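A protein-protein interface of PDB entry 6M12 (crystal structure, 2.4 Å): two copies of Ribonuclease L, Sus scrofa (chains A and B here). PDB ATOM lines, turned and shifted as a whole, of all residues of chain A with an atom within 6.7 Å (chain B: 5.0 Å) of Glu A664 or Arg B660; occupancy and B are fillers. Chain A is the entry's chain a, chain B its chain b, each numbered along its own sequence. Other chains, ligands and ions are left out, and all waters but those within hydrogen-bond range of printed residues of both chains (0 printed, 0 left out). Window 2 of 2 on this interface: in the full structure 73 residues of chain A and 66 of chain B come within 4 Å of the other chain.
Of the printed residues of chain B, Asn A583 touches Glu B664.
Gly A663 touches none of the printed residues of chain B.
Glu A664 touches four residues of chain B.
Printed residues of chain B within 4 Å of Glu A668: Lys B588 (3.1 Å).
Of chain A, only Glu A664 (3.0 Å) comes within 4 Å of Arg B660.
The nearest printed residue of chain B that does not touch Glu A664 is Arg B579 (6.4 Å).
The nearest printed residue of chain A that does not touch Asn B583 is Gly A663 (4.6 Å).
Among the printed residues, merely in contact across the chains: Glu A664 with Glu B664 (3.5 Å) and Glu A664 with Lys B588 (3.7 Å).
Along chain B the printed residues that touch a printed residue of chain A span positions 583 to 664.
Among the printed residues, Asp or Glu carboxylates within 4 Å of a Lys or Arg side-chain nitrogen of the other chain: Arg A660 with Glu B664 (3.0 Å), Glu A664 with Arg B660 (3.0 Å) and Glu A668 with Lys B588 (3.1 Å).
Asn A583 touches Glu B664, and with the chains exchanged Glu A664 touches Asn B583.
Arg A660 touches Glu B664, and with the chains exchanged Glu A664 touches Arg B660.
Glu B664 touches its own counterpart, Glu A664.
Positions printed for both chains: 579, 583, 659, 660, 661, 662, 663, 664 and 665.
The side-chain amide nitrogen (ND2) of Asn A583 sits at hydrogen-bond distance from the backbone carbonyl oxygen (O) of Glu B664 (3.0 Å).
The side-chain amide nitrogen (ND2) of Asn B583 is in hydrogen-bond range of the backbone carbonyl oxygen (O) of Glu A664 (3.1 Å).
OE1 of Glu A664 lies within salt-bridge range of NH1 of Arg B660 (3.0 Å).
OE2 of Glu A668 lies within salt-bridge range of NZ of Lys B588, at 3.1 Å.
The guanidinium group (NH1) of Arg A660 lies within salt-bridge range of the side-chain carboxylate (OE1) of Glu B664.
The side-chain amide oxygen (OD1) of Asn A661 is in hydrogen-bond range of the guanidinium group (NE) of Arg A660 (3.1 Å).
ND1 of His A665 is in hydrogen-bond range of OE2 of Glu A668, 3.0 Å away.
OE2 of Glu B664 lies within salt-bridge range of NH2 of Arg B579.
The guanidinium group of Arg A660 lies within hydrogen-bond range of the side-chain amide oxygen of Asn A583 (2.8 Å).
NH2 of Arg A579 is in salt-bridge range of OE2 of Glu A664, 2.8 Å away.
NE of Arg B660 sits at hydrogen-bond distance from OD1 of Asn B661, 3.1 Å away.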
ATOM      1  N   TYR A 575     -25.559  -5.321 -21.380  1.00  0.00           N
ATOM      2  CA  TYR A 575     -24.967  -6.235 -22.370  1.00  0.00           C
ATOM      3  C   TYR A 575     -24.536  -7.586 -21.726  1.00  0.00           C
ATOM      4  O   TYR A 575     -24.902  -8.657 -22.182  1.00  0.00           O
ATOM      5  CB  TYR A 575     -23.816  -5.532 -23.017  1.00  0.00           C
ATOM      6  CG  TYR A 575     -23.026  -6.276 -24.057  1.00  0.00           C
ATOM      7  CD1 TYR A 575     -23.637  -6.922 -25.109  1.00  0.00           C
ATOM      8  CD2 TYR A 575     -21.628  -6.217 -24.046  1.00  0.00           C
ATOM      9  CE1 TYR A 575     -22.874  -7.545 -26.107  1.00  0.00           C
ATOM     10  CE2 TYR A 575     -20.867  -6.842 -25.018  1.00  0.00           C
ATOM     11  CZ  TYR A 575     -21.477  -7.497 -26.036  1.00  0.00           C
ATOM     12  OH  TYR A 575     -20.677  -8.088 -26.952  1.00  0.00           O
ATOM     13  N   ARG A 576     -23.859  -7.502 -20.608  1.00  0.00           N
ATOM     14  CA  ARG A 576     -23.456  -8.686 -19.840  1.00  0.00           C
ATOM     15  C   ARG A 576     -24.627  -9.568 -19.471  1.00  0.00           C
ATOM     16  O   ARG A 576     -24.535 -10.790 -19.547  1.00  0.00           O
ATOM     17  CB  ARG A 576     -22.747  -8.219 -18.557  1.00  0.00           C
ATOM     18  CG  ARG A 576     -22.132  -9.312 -17.710  1.00  0.00           C
ATOM     19  CD  ARG A 576     -20.939  -9.978 -18.420  1.00  0.00           C
ATOM     20  NE  ARG A 576     -21.357 -11.080 -19.273  1.00  0.00           N
ATOM     21  CZ  ARG A 576     -20.540 -11.860 -20.005  1.00  0.00           C
ATOM     22  NH1 ARG A 576     -19.210 -11.683 -20.035  1.00  0.00           N
ATOM     23  NH2 ARG A 576     -21.065 -12.829 -20.728  1.00  0.00           N
ATOM     24  N   ARG A 579     -26.108 -11.240 -22.626  1.00  0.00           N
ATOM     25  CA  ARG A 579     -25.196 -12.318 -22.990  1.00  0.00           C
ATOM     26  C   ARG A 579     -25.363 -13.556 -22.099  1.00  0.00           C
ATOM     27  O   ARG A 579     -25.406 -14.657 -22.588  1.00  0.00           O
ATOM     28  CB  ARG A 579     -23.742 -11.849 -22.919  1.00  0.00           C
ATOM     29  CG  ARG A 579     -23.381 -10.848 -24.007  1.00  0.00           C
ATOM     30  CD  ARG A 579     -22.077 -10.149 -23.730  1.00  0.00           C
ATOM     31  NE  ARG A 579     -20.957 -11.054 -23.856  1.00  0.00           N
ATOM     32  CZ  ARG A 579     -19.688 -10.722 -23.627  1.00  0.00           C
ATOM     33  NH1 ARG A 579     -19.363  -9.497 -23.242  1.00  0.00           N
ATOM     34  NH2 ARG A 579     -18.742 -11.634 -23.790  1.00  0.00           N
ATOM     35  N   ASN A 583     -26.774 -17.559 -22.974  1.00  0.00           N
ATOM     36  CA  ASN A 583     -25.902 -18.695 -22.834  1.00  0.00           C
ATOM     37  C   ASN A 583     -26.563 -19.811 -22.029  1.00  0.00           C
ATOM     38  O   ASN A 583     -25.920 -20.810 -21.673  1.00  0.00           O
ATOM     39  CB  ASN A 583     -24.639 -18.255 -22.081  1.00  0.00           C
ATOM     40  CG  ASN A 583     -23.531 -19.276 -22.177  1.00  0.00           C
ATOM     41  OD1 ASN A 583     -23.104 -19.610 -23.265  1.00  0.00           O
ATOM     42  ND2 ASN A 583     -23.108 -19.799 -21.054  1.00  0.00           N
ATOM     43  N   ILE A 659     -26.784 -12.455 -29.312  1.00  0.00           N
ATOM     44  CA  ILE A 659     -26.045 -11.509 -28.536  1.00  0.00           C
ATOM     45  C   ILE A 659     -24.913 -12.225 -27.823  1.00  0.00           C
ATOM     46  O   ILE A 659     -23.764 -11.777 -27.878  1.00  0.00           O
ATOM     47  CB  ILE A 659     -26.976 -10.704 -27.609  1.00  0.00           C
ATOM     48  CG1 ILE A 659     -27.762  -9.703 -28.475  1.00  0.00           C
ATOM     49  CG2 ILE A 659     -26.160  -9.909 -26.594  1.00  0.00           C
ATOM     50  CD1 ILE A 659     -28.927  -9.017 -27.783  1.00  0.00           C
ATOM     51  N   ARG A 660     -25.227 -13.369 -27.238  1.00  0.00           N
ATOM     52  CA  ARG A 660     -24.224 -14.189 -26.586  1.00  0.00           C
ATOM     53  C   ARG A 660     -23.051 -14.546 -27.488  1.00  0.00           C
ATOM     54  O   ARG A 660     -21.897 -14.371 -27.095  1.00  0.00           O
ATOM     55  CB  ARG A 660     -24.854 -15.490 -26.080  1.00  0.00           C
ATOM     56  CG  ARG A 660     -23.926 -16.249 -25.152  1.00  0.00           C
ATOM     57  CD  ARG A 660     -23.715 -17.697 -25.514  1.00  0.00           C
ATOM     58  NE  ARG A 660     -22.720 -17.879 -26.556  1.00  0.00           N
ATOM     59  CZ  ARG A 660     -21.611 -18.626 -26.467  1.00  0.00           C
ATOM     60  NH1 ARG A 660     -21.259 -19.284 -25.370  1.00  0.00           N
ATOM     61  NH2 ARG A 660     -20.823 -18.707 -27.519  1.00  0.00           N
ATOM     62  N   ASN A 661     -23.368 -15.057 -28.677  1.00  0.00           N
ATOM     63  CA  ASN A 661     -22.352 -15.536 -29.645  1.00  0.00           C
ATOM     64  C   ASN A 661     -21.475 -14.403 -30.135  1.00  0.00           C
ATOM     65  O   ASN A 661     -20.240 -14.546 -30.203  1.00  0.00           O
ATOM     66  CB  ASN A 661     -22.988 -16.224 -30.871  1.00  0.00           C
ATOM     67  CG  ASN A 661     -23.611 -17.567 -30.541  1.00  0.00           C
ATOM     68  OD1 ASN A 661     -23.214 -18.239 -29.577  1.00  0.00           O
ATOM     69  ND2 ASN A 661     -24.645 -17.958 -31.324  1.00  0.00           N
ATOM     70  N   LEU A 662     -22.101 -13.282 -30.474  1.00  0.00           N
ATOM     71  CA  LEU A 662     -21.342 -12.119 -30.918  1.00  0.00           C
ATOM     72  C   LEU A 662     -20.463 -11.634 -29.801  1.00  0.00           C
ATOM     73  O   LEU A 662     -19.318 -11.297 -30.029  1.00  0.00           O
ATOM     74  CB  LEU A 662     -22.276 -11.013 -31.322  1.00  0.00           C
ATOM     75  CG  LEU A 662     -21.625  -9.857 -32.070  1.00  0.00           C
ATOM     76  CD1 LEU A 662     -22.577  -9.269 -33.108  1.00  0.00           C
ATOM     77  CD2 LEU A 662     -21.171  -8.766 -31.119  1.00  0.00           C
ATOM     78  N   GLY A 663     -21.030 -11.605 -28.595  1.00  0.00           N
ATOM     79  CA  GLY A 663     -20.278 -11.308 -27.396  1.00  0.00           C
ATOM     80  C   GLY A 663     -18.957 -12.058 -27.343  1.00  0.00           C
ATOM     81  O   GLY A 663     -17.892 -11.448 -27.211  1.00  0.00           O
ATOM     82  N   GLU A 664     -19.027 -13.370 -27.522  1.00  0.00           N
ATOM     83  CA  GLU A 664     -17.844 -14.184 -27.376  1.00  0.00           C
ATOM     84  C   GLU A 664     -16.821 -14.019 -28.515  1.00  0.00           C
ATOM     85  O   GLU A 664     -15.607 -14.033 -28.254  1.00  0.00           O
ATOM     86  CB  GLU A 664     -18.220 -15.637 -27.227  1.00  0.00           C
ATOM     87  CG  GLU A 664     -18.901 -15.988 -25.927  1.00  0.00           C
ATOM     88  CD  GLU A 664     -18.180 -15.490 -24.693  1.00  0.00           C
ATOM     89  OE1 GLU A 664     -17.208 -16.130 -24.259  1.00  0.00           O
ATOM     90  OE2 GLU A 664     -18.613 -14.457 -24.152  1.00  0.00           O
ATOM     91  N   HIS A 665     -17.293 -13.838 -29.743  1.00  0.00           N
ATOM     92  CA  HIS A 665     -16.419 -13.989 -30.919  1.00  0.00           C
ATOM     93  C   HIS A 665     -16.106 -12.668 -31.625  1.00  0.00           C
ATOM     94  O   HIS A 665     -15.254 -12.647 -32.499  1.00  0.00           O
ATOM     95  CB  HIS A 665     -17.030 -14.973 -31.931  1.00  0.00           C
ATOM     96  CG  HIS A 665     -17.421 -16.293 -31.355  1.00  0.00           C
ATOM     97  ND1 HIS A 665     -16.555 -17.053 -30.609  1.00  0.00           N
ATOM     98  CD2 HIS A 665     -18.569 -17.006 -31.447  1.00  0.00           C
ATOM     99  CE1 HIS A 665     -17.164 -18.161 -30.229  1.00  0.00           C
ATOM    100  NE2 HIS A 665     -18.385 -18.164 -30.732  1.00  0.00           N
ATOM    101  N   ILE A 666     -16.765 -11.580 -31.244  1.00  0.00           N
ATOM    102  CA  ILE A 666     -16.583 -10.274 -31.880  1.00  0.00           C
ATOM    103  C   ILE A 666     -15.128  -9.828 -32.050  1.00  0.00           C
ATOM    104  O   ILE A 666     -14.822  -9.082 -32.986  1.00  0.00           O
ATOM    105  CB  ILE A 666     -17.375  -9.164 -31.102  1.00  0.00           C
ATOM    106  CG1 ILE A 666     -17.541  -7.878 -31.917  1.00  0.00           C
ATOM    107  CG2 ILE A 666     -16.715  -8.857 -29.762  1.00  0.00           C
ATOM    108  CD1 ILE A 666     -18.319  -8.086 -33.203  1.00  0.00           C
ATOM    109  N   ASN A 667     -14.256 -10.243 -31.139  1.00  0.00           N
ATOM    110  CA  ASN A 667     -12.856  -9.777 -31.130  1.00  0.00           C
ATOM    111  C   ASN A 667     -11.858 -10.722 -31.786  1.00  0.00           C
ATOM    112  O   ASN A 667     -10.663 -10.448 -31.795  1.00  0.00           O
ATOM    113  CB  ASN A 667     -12.404  -9.514 -29.700  1.00  0.00           C
ATOM    114  CG  ASN A 667     -12.937  -8.222 -29.171  1.00  0.00           C
ATOM    115  OD1 ASN A 667     -12.715  -7.176 -29.753  1.00  0.00           O
ATOM    116  ND2 ASN A 667     -13.664  -8.284 -28.066  1.00  0.00           N
ATOM    117  N   GLU A 668     -12.344 -11.856 -32.289  1.00  0.00           N
ATOM    118  CA  GLU A 668     -11.534 -12.769 -33.081  1.00  0.00           C
ATOM    119  C   GLU A 668     -11.244 -12.103 -34.415  1.00  0.00           C
ATOM    120  O   GLU A 668     -12.048 -11.318 -34.941  1.00  0.00           O
ATOM    121  CB  GLU A 668     -12.220 -14.111 -33.279  1.00  0.00           C
ATOM    122  CG  GLU A 668     -12.378 -14.885 -31.992  1.00  0.00           C
ATOM    123  CD  GLU A 668     -13.204 -16.145 -32.153  1.00  0.00           C
ATOM    124  OE1 GLU A 668     -13.477 -16.537 -33.300  1.00  0.00           O
ATOM    125  OE2 GLU A 668     -13.617 -16.741 -31.129  1.00  0.00           O
ATOM    126  N   ARG B 579     -12.101 -15.503 -16.700  1.00  0.00           N
ATOM    127  CA  ARG B 579     -12.801 -15.886 -17.919  1.00  0.00           C
ATOM    128  C   ARG B 579     -12.588 -14.885 -19.044  1.00  0.00           C
ATOM    129  O   ARG B 579     -12.362 -15.264 -20.179  1.00  0.00           O
ATOM    130  CB  ARG B 579     -14.304 -16.053 -17.663  1.00  0.00           C
ATOM    131  CG  ARG B 579     -14.652 -17.242 -16.785  1.00  0.00           C
ATOM    132  CD  ARG B 579     -16.079 -17.188 -16.255  1.00  0.00           C
ATOM    133  NE  ARG B 579     -17.023 -17.413 -17.338  1.00  0.00           N
ATOM    134  CZ  ARG B 579     -18.346 -17.390 -17.197  1.00  0.00           C
ATOM    135  NH1 ARG B 579     -18.898 -17.177 -16.001  1.00  0.00           N
ATOM    136  NH2 ARG B 579     -19.117 -17.606 -18.252  1.00  0.00           N
ATOM    137  N   GLY B 582      -9.117 -15.021 -20.483  1.00  0.00           N
ATOM    138  CA  GLY B 582      -9.058 -16.250 -21.292  1.00  0.00           C
ATOM    139  C   GLY B 582      -9.873 -16.295 -22.574  1.00  0.00           C
ATOM    140  O   GLY B 582      -9.867 -17.302 -23.250  1.00  0.00           O
ATOM    141  N   ASN B 583     -10.602 -15.232 -22.883  1.00  0.00           N
ATOM    142  CA  ASN B 583     -11.351 -15.115 -24.120  1.00  0.00           C
ATOM    143  C   ASN B 583     -10.662 -14.157 -25.078  1.00  0.00           C
ATOM    144  O   ASN B 583     -11.205 -13.840 -26.155  1.00  0.00           O
ATOM    145  CB  ASN B 583     -12.756 -14.556 -23.804  1.00  0.00           C
ATOM    146  CG  ASN B 583     -13.699 -14.686 -24.974  1.00  0.00           C
ATOM    147  OD1 ASN B 583     -13.963 -15.785 -25.416  1.00  0.00           O
ATOM    148  ND2 ASN B 583     -14.143 -13.571 -25.530  1.00  0.00           N
ATOM    149  N   LYS B 588      -6.682 -17.783 -27.099  1.00  0.00           N
ATOM    150  CA  LYS B 588      -7.391 -18.883 -27.756  1.00  0.00           C
ATOM    151  C   LYS B 588      -6.592 -19.490 -28.907  1.00  0.00           C
ATOM    152  O   LYS B 588      -6.495 -20.719 -29.013  1.00  0.00           O
ATOM    153  CB  LYS B 588      -8.790 -18.450 -28.213  1.00  0.00           C
ATOM    154  CG  LYS B 588      -9.753 -18.352 -27.016  1.00  0.00           C
ATOM    155  CD  LYS B 588     -11.178 -17.871 -27.306  1.00  0.00           C
ATOM    156  CE  LYS B 588     -11.181 -16.681 -28.241  1.00  0.00           C
ATOM    157  NZ  LYS B 588     -12.497 -16.017 -28.316  1.00  0.00           N
ATOM    158  N   LEU B 655      -4.516 -22.195 -19.200  1.00  0.00           N
ATOM    159  CA  LEU B 655      -5.358 -22.277 -18.003  1.00  0.00           C
ATOM    160  C   LEU B 655      -6.499 -21.262 -18.083  1.00  0.00           C
ATOM    161  O   LEU B 655      -7.637 -21.587 -17.798  1.00  0.00           O
ATOM    162  CB  LEU B 655      -4.567 -22.014 -16.726  1.00  0.00           C
ATOM    163  CG  LEU B 655      -5.000 -22.786 -15.492  1.00  0.00           C
ATOM    164  CD1 LEU B 655      -4.474 -22.150 -14.226  1.00  0.00           C
ATOM    165  CD2 LEU B 655      -6.483 -22.942 -15.313  1.00  0.00           C
ATOM    166  N   LEU B 656      -6.163 -20.040 -18.473  1.00  0.00           N
ATOM    167  CA  LEU B 656      -7.154 -18.997 -18.652  1.00  0.00           C
ATOM    168  C   LEU B 656      -8.141 -19.406 -19.703  1.00  0.00           C
ATOM    169  O   LEU B 656      -9.346 -19.313 -19.481  1.00  0.00           O
ATOM    170  CB  LEU B 656      -6.484 -17.661 -18.967  1.00  0.00           C
ATOM    171  CG  LEU B 656      -5.967 -16.819 -17.788  1.00  0.00           C
ATOM    172  CD1 LEU B 656      -6.021 -17.481 -16.445  1.00  0.00           C
ATOM    173  CD2 LEU B 656      -4.557 -16.360 -18.058  1.00  0.00           C
ATOM    174  N   LYS B 657      -7.629 -19.937 -20.807  1.00  0.00           N
ATOM    175  CA  LYS B 657      -8.480 -20.509 -21.868  1.00  0.00           C
ATOM    176  C   LYS B 657      -9.388 -21.599 -21.315  1.00  0.00           C
ATOM    177  O   LYS B 657     -10.559 -21.662 -21.639  1.00  0.00           O
ATOM    178  CB  LYS B 657      -7.625 -21.071 -22.988  1.00  0.00           C
ATOM    179  CG  LYS B 657      -8.407 -21.810 -24.061  1.00  0.00           C
ATOM    180  CD  LYS B 657      -7.826 -21.681 -25.455  1.00  0.00           C
ATOM    181  CE  LYS B 657      -7.300 -23.005 -26.026  1.00  0.00           C
ATOM    182  NZ  LYS B 657      -5.981 -23.491 -25.492  1.00  0.00           N
ATOM    183  N   PHE B 658      -8.836 -22.454 -20.489  1.00  0.00           N
ATOM    184  CA  PHE B 658      -9.585 -23.533 -19.878  1.00  0.00           C
ATOM    185  C   PHE B 658     -10.711 -22.969 -19.028  1.00  0.00           C
ATOM    186  O   PHE B 658     -11.839 -23.452 -19.083  1.00  0.00           O
ATOM    187  CB  PHE B 658      -8.631 -24.389 -19.029  1.00  0.00           C
ATOM    188  CG  PHE B 658      -9.268 -25.587 -18.386  1.00  0.00           C
ATOM    189  CD1 PHE B 658      -9.385 -26.779 -19.077  1.00  0.00           C
ATOM    190  CD2 PHE B 658      -9.675 -25.539 -17.058  1.00  0.00           C
ATOM    191  CE1 PHE B 658      -9.923 -27.874 -18.464  1.00  0.00           C
ATOM    192  CE2 PHE B 658     -10.259 -26.642 -16.459  1.00  0.00           C
ATOM    193  CZ  PHE B 658     -10.388 -27.823 -17.172  1.00  0.00           C
ATOM    194  N   ILE B 659     -10.400 -21.934 -18.255  1.00  0.00           N
ATOM    195  CA  ILE B 659     -11.361 -21.349 -17.357  1.00  0.00           C
ATOM    196  C   ILE B 659     -12.477 -20.713 -18.193  1.00  0.00           C
ATOM    197  O   ILE B 659     -13.652 -20.947 -17.932  1.00  0.00           O
ATOM    198  CB  ILE B 659     -10.669 -20.394 -16.384  1.00  0.00           C
ATOM    199  CG1 ILE B 659      -9.891 -21.235 -15.345  1.00  0.00           C
ATOM    200  CG2 ILE B 659     -11.705 -19.544 -15.651  1.00  0.00           C
ATOM    201  CD1 ILE B 659      -8.971 -20.472 -14.417  1.00  0.00           C
ATOM    202  N   ARG B 660     -12.105 -19.991 -19.240  1.00  0.00           N
ATOM    203  CA  ARG B 660     -13.062 -19.417 -20.149  1.00  0.00           C
ATOM    204  C   ARG B 660     -14.032 -20.434 -20.733  1.00  0.00           C
ATOM    205  O   ARG B 660     -15.238 -20.222 -20.699  1.00  0.00           O
ATOM    206  CB  ARG B 660     -12.350 -18.722 -21.318  1.00  0.00           C
ATOM    207  CG  ARG B 660     -13.297 -17.859 -22.134  1.00  0.00           C
ATOM    208  CD  ARG B 660     -13.274 -18.109 -23.610  1.00  0.00           C
ATOM    209  NE  ARG B 660     -14.080 -19.251 -24.007  1.00  0.00           N
ATOM    210  CZ  ARG B 660     -15.037 -19.254 -24.951  1.00  0.00           C
ATOM    211  NH1 ARG B 660     -15.436 -18.159 -25.599  1.00  0.00           N
ATOM    212  NH2 ARG B 660     -15.651 -20.402 -25.232  1.00  0.00           N
ATOM    213  N   ASN B 661     -13.487 -21.514 -21.281  1.00  0.00           N
ATOM    214  CA  ASN B 661     -14.271 -22.559 -21.968  1.00  0.00           C
ATOM    215  C   ASN B 661     -15.203 -23.286 -21.006  1.00  0.00           C
ATOM    216  O   ASN B 661     -16.375 -23.530 -21.336  1.00  0.00           O
ATOM    217  CB  ASN B 661     -13.368 -23.608 -22.625  1.00  0.00           C
ATOM    218  CG  ASN B 661     -12.637 -23.085 -23.847  1.00  0.00           C
ATOM    219  OD1 ASN B 661     -13.089 -22.142 -24.516  1.00  0.00           O
ATOM    220  ND2 ASN B 661     -11.479 -23.698 -24.145  1.00  0.00           N
ATOM    221  N   LEU B 662     -14.689 -23.626 -19.830  1.00  0.00           N
ATOM    222  CA  LEU B 662     -15.520 -24.260 -18.818  1.00  0.00           C
ATOM    223  C   LEU B 662     -16.609 -23.322 -18.396  1.00  0.00           C
ATOM    224  O   LEU B 662     -17.735 -23.723 -18.230  1.00  0.00           O
ATOM    225  CB  LEU B 662     -14.693 -24.629 -17.613  1.00  0.00           C
ATOM    226  CG  LEU B 662     -15.409 -25.561 -16.621  1.00  0.00           C
ATOM    227  CD1 LEU B 662     -14.392 -26.540 -16.007  1.00  0.00           C
ATOM    228  CD2 LEU B 662     -16.110 -24.751 -15.535  1.00  0.00           C
ATOM    229  N   GLY B 663     -16.243 -22.062 -18.216  1.00  0.00           N
ATOM    230  CA  GLY B 663     -17.191 -20.995 -17.944  1.00  0.00           C
ATOM    231  C   GLY B 663     -18.369 -21.048 -18.869  1.00  0.00           C
ATOM    232  O   GLY B 663     -19.497 -21.084 -18.415  1.00  0.00           O
ATOM    233  N   GLU B 664     -18.105 -21.124 -20.166  1.00  0.00           N
ATOM    234  CA  GLU B 664     -19.167 -21.080 -21.138  1.00  0.00           C
ATOM    235  C   GLU B 664     -20.036 -22.325 -21.175  1.00  0.00           C
ATOM    236  O   GLU B 664     -21.265 -22.208 -21.347  1.00  0.00           O
ATOM    237  CB  GLU B 664     -18.616 -20.777 -22.525  1.00  0.00           C
ATOM    238  CG  GLU B 664     -18.083 -19.357 -22.687  1.00  0.00           C
ATOM    239  CD  GLU B 664     -19.043 -18.271 -22.198  1.00  0.00           C
ATOM    240  OE1 GLU B 664     -20.054 -17.957 -22.903  1.00  0.00           O
ATOM    241  OE2 GLU B 664     -18.773 -17.758 -21.088  1.00  0.00           O
ATOM    242  N   HIS B 665     -19.433 -23.501 -20.984  1.00  0.00           N
ATOM    243  CA  HIS B 665     -20.102 -24.770 -21.302  1.00  0.00           C
ATOM    244  C   HIS B 665     -20.489 -25.591 -20.083  1.00  0.00           C
ATOM    245  O   HIS B 665     -21.227 -26.551 -20.210  1.00  0.00           O
ATOM    246  CB  HIS B 665     -19.224 -25.612 -22.253  1.00  0.00           C
ATOM    247  CG  HIS B 665     -18.808 -24.878 -23.491  1.00  0.00           C
ATOM    248  ND1 HIS B 665     -19.723 -24.244 -24.309  1.00  0.00           N
ATOM    249  CD2 HIS B 665     -17.602 -24.698 -24.071  1.00  0.00           C
ATOM    250  CE1 HIS B 665     -19.104 -23.694 -25.332  1.00  0.00           C
ATOM    251  NE2 HIS B 665     -17.808 -23.923 -25.195  1.00  0.00           N
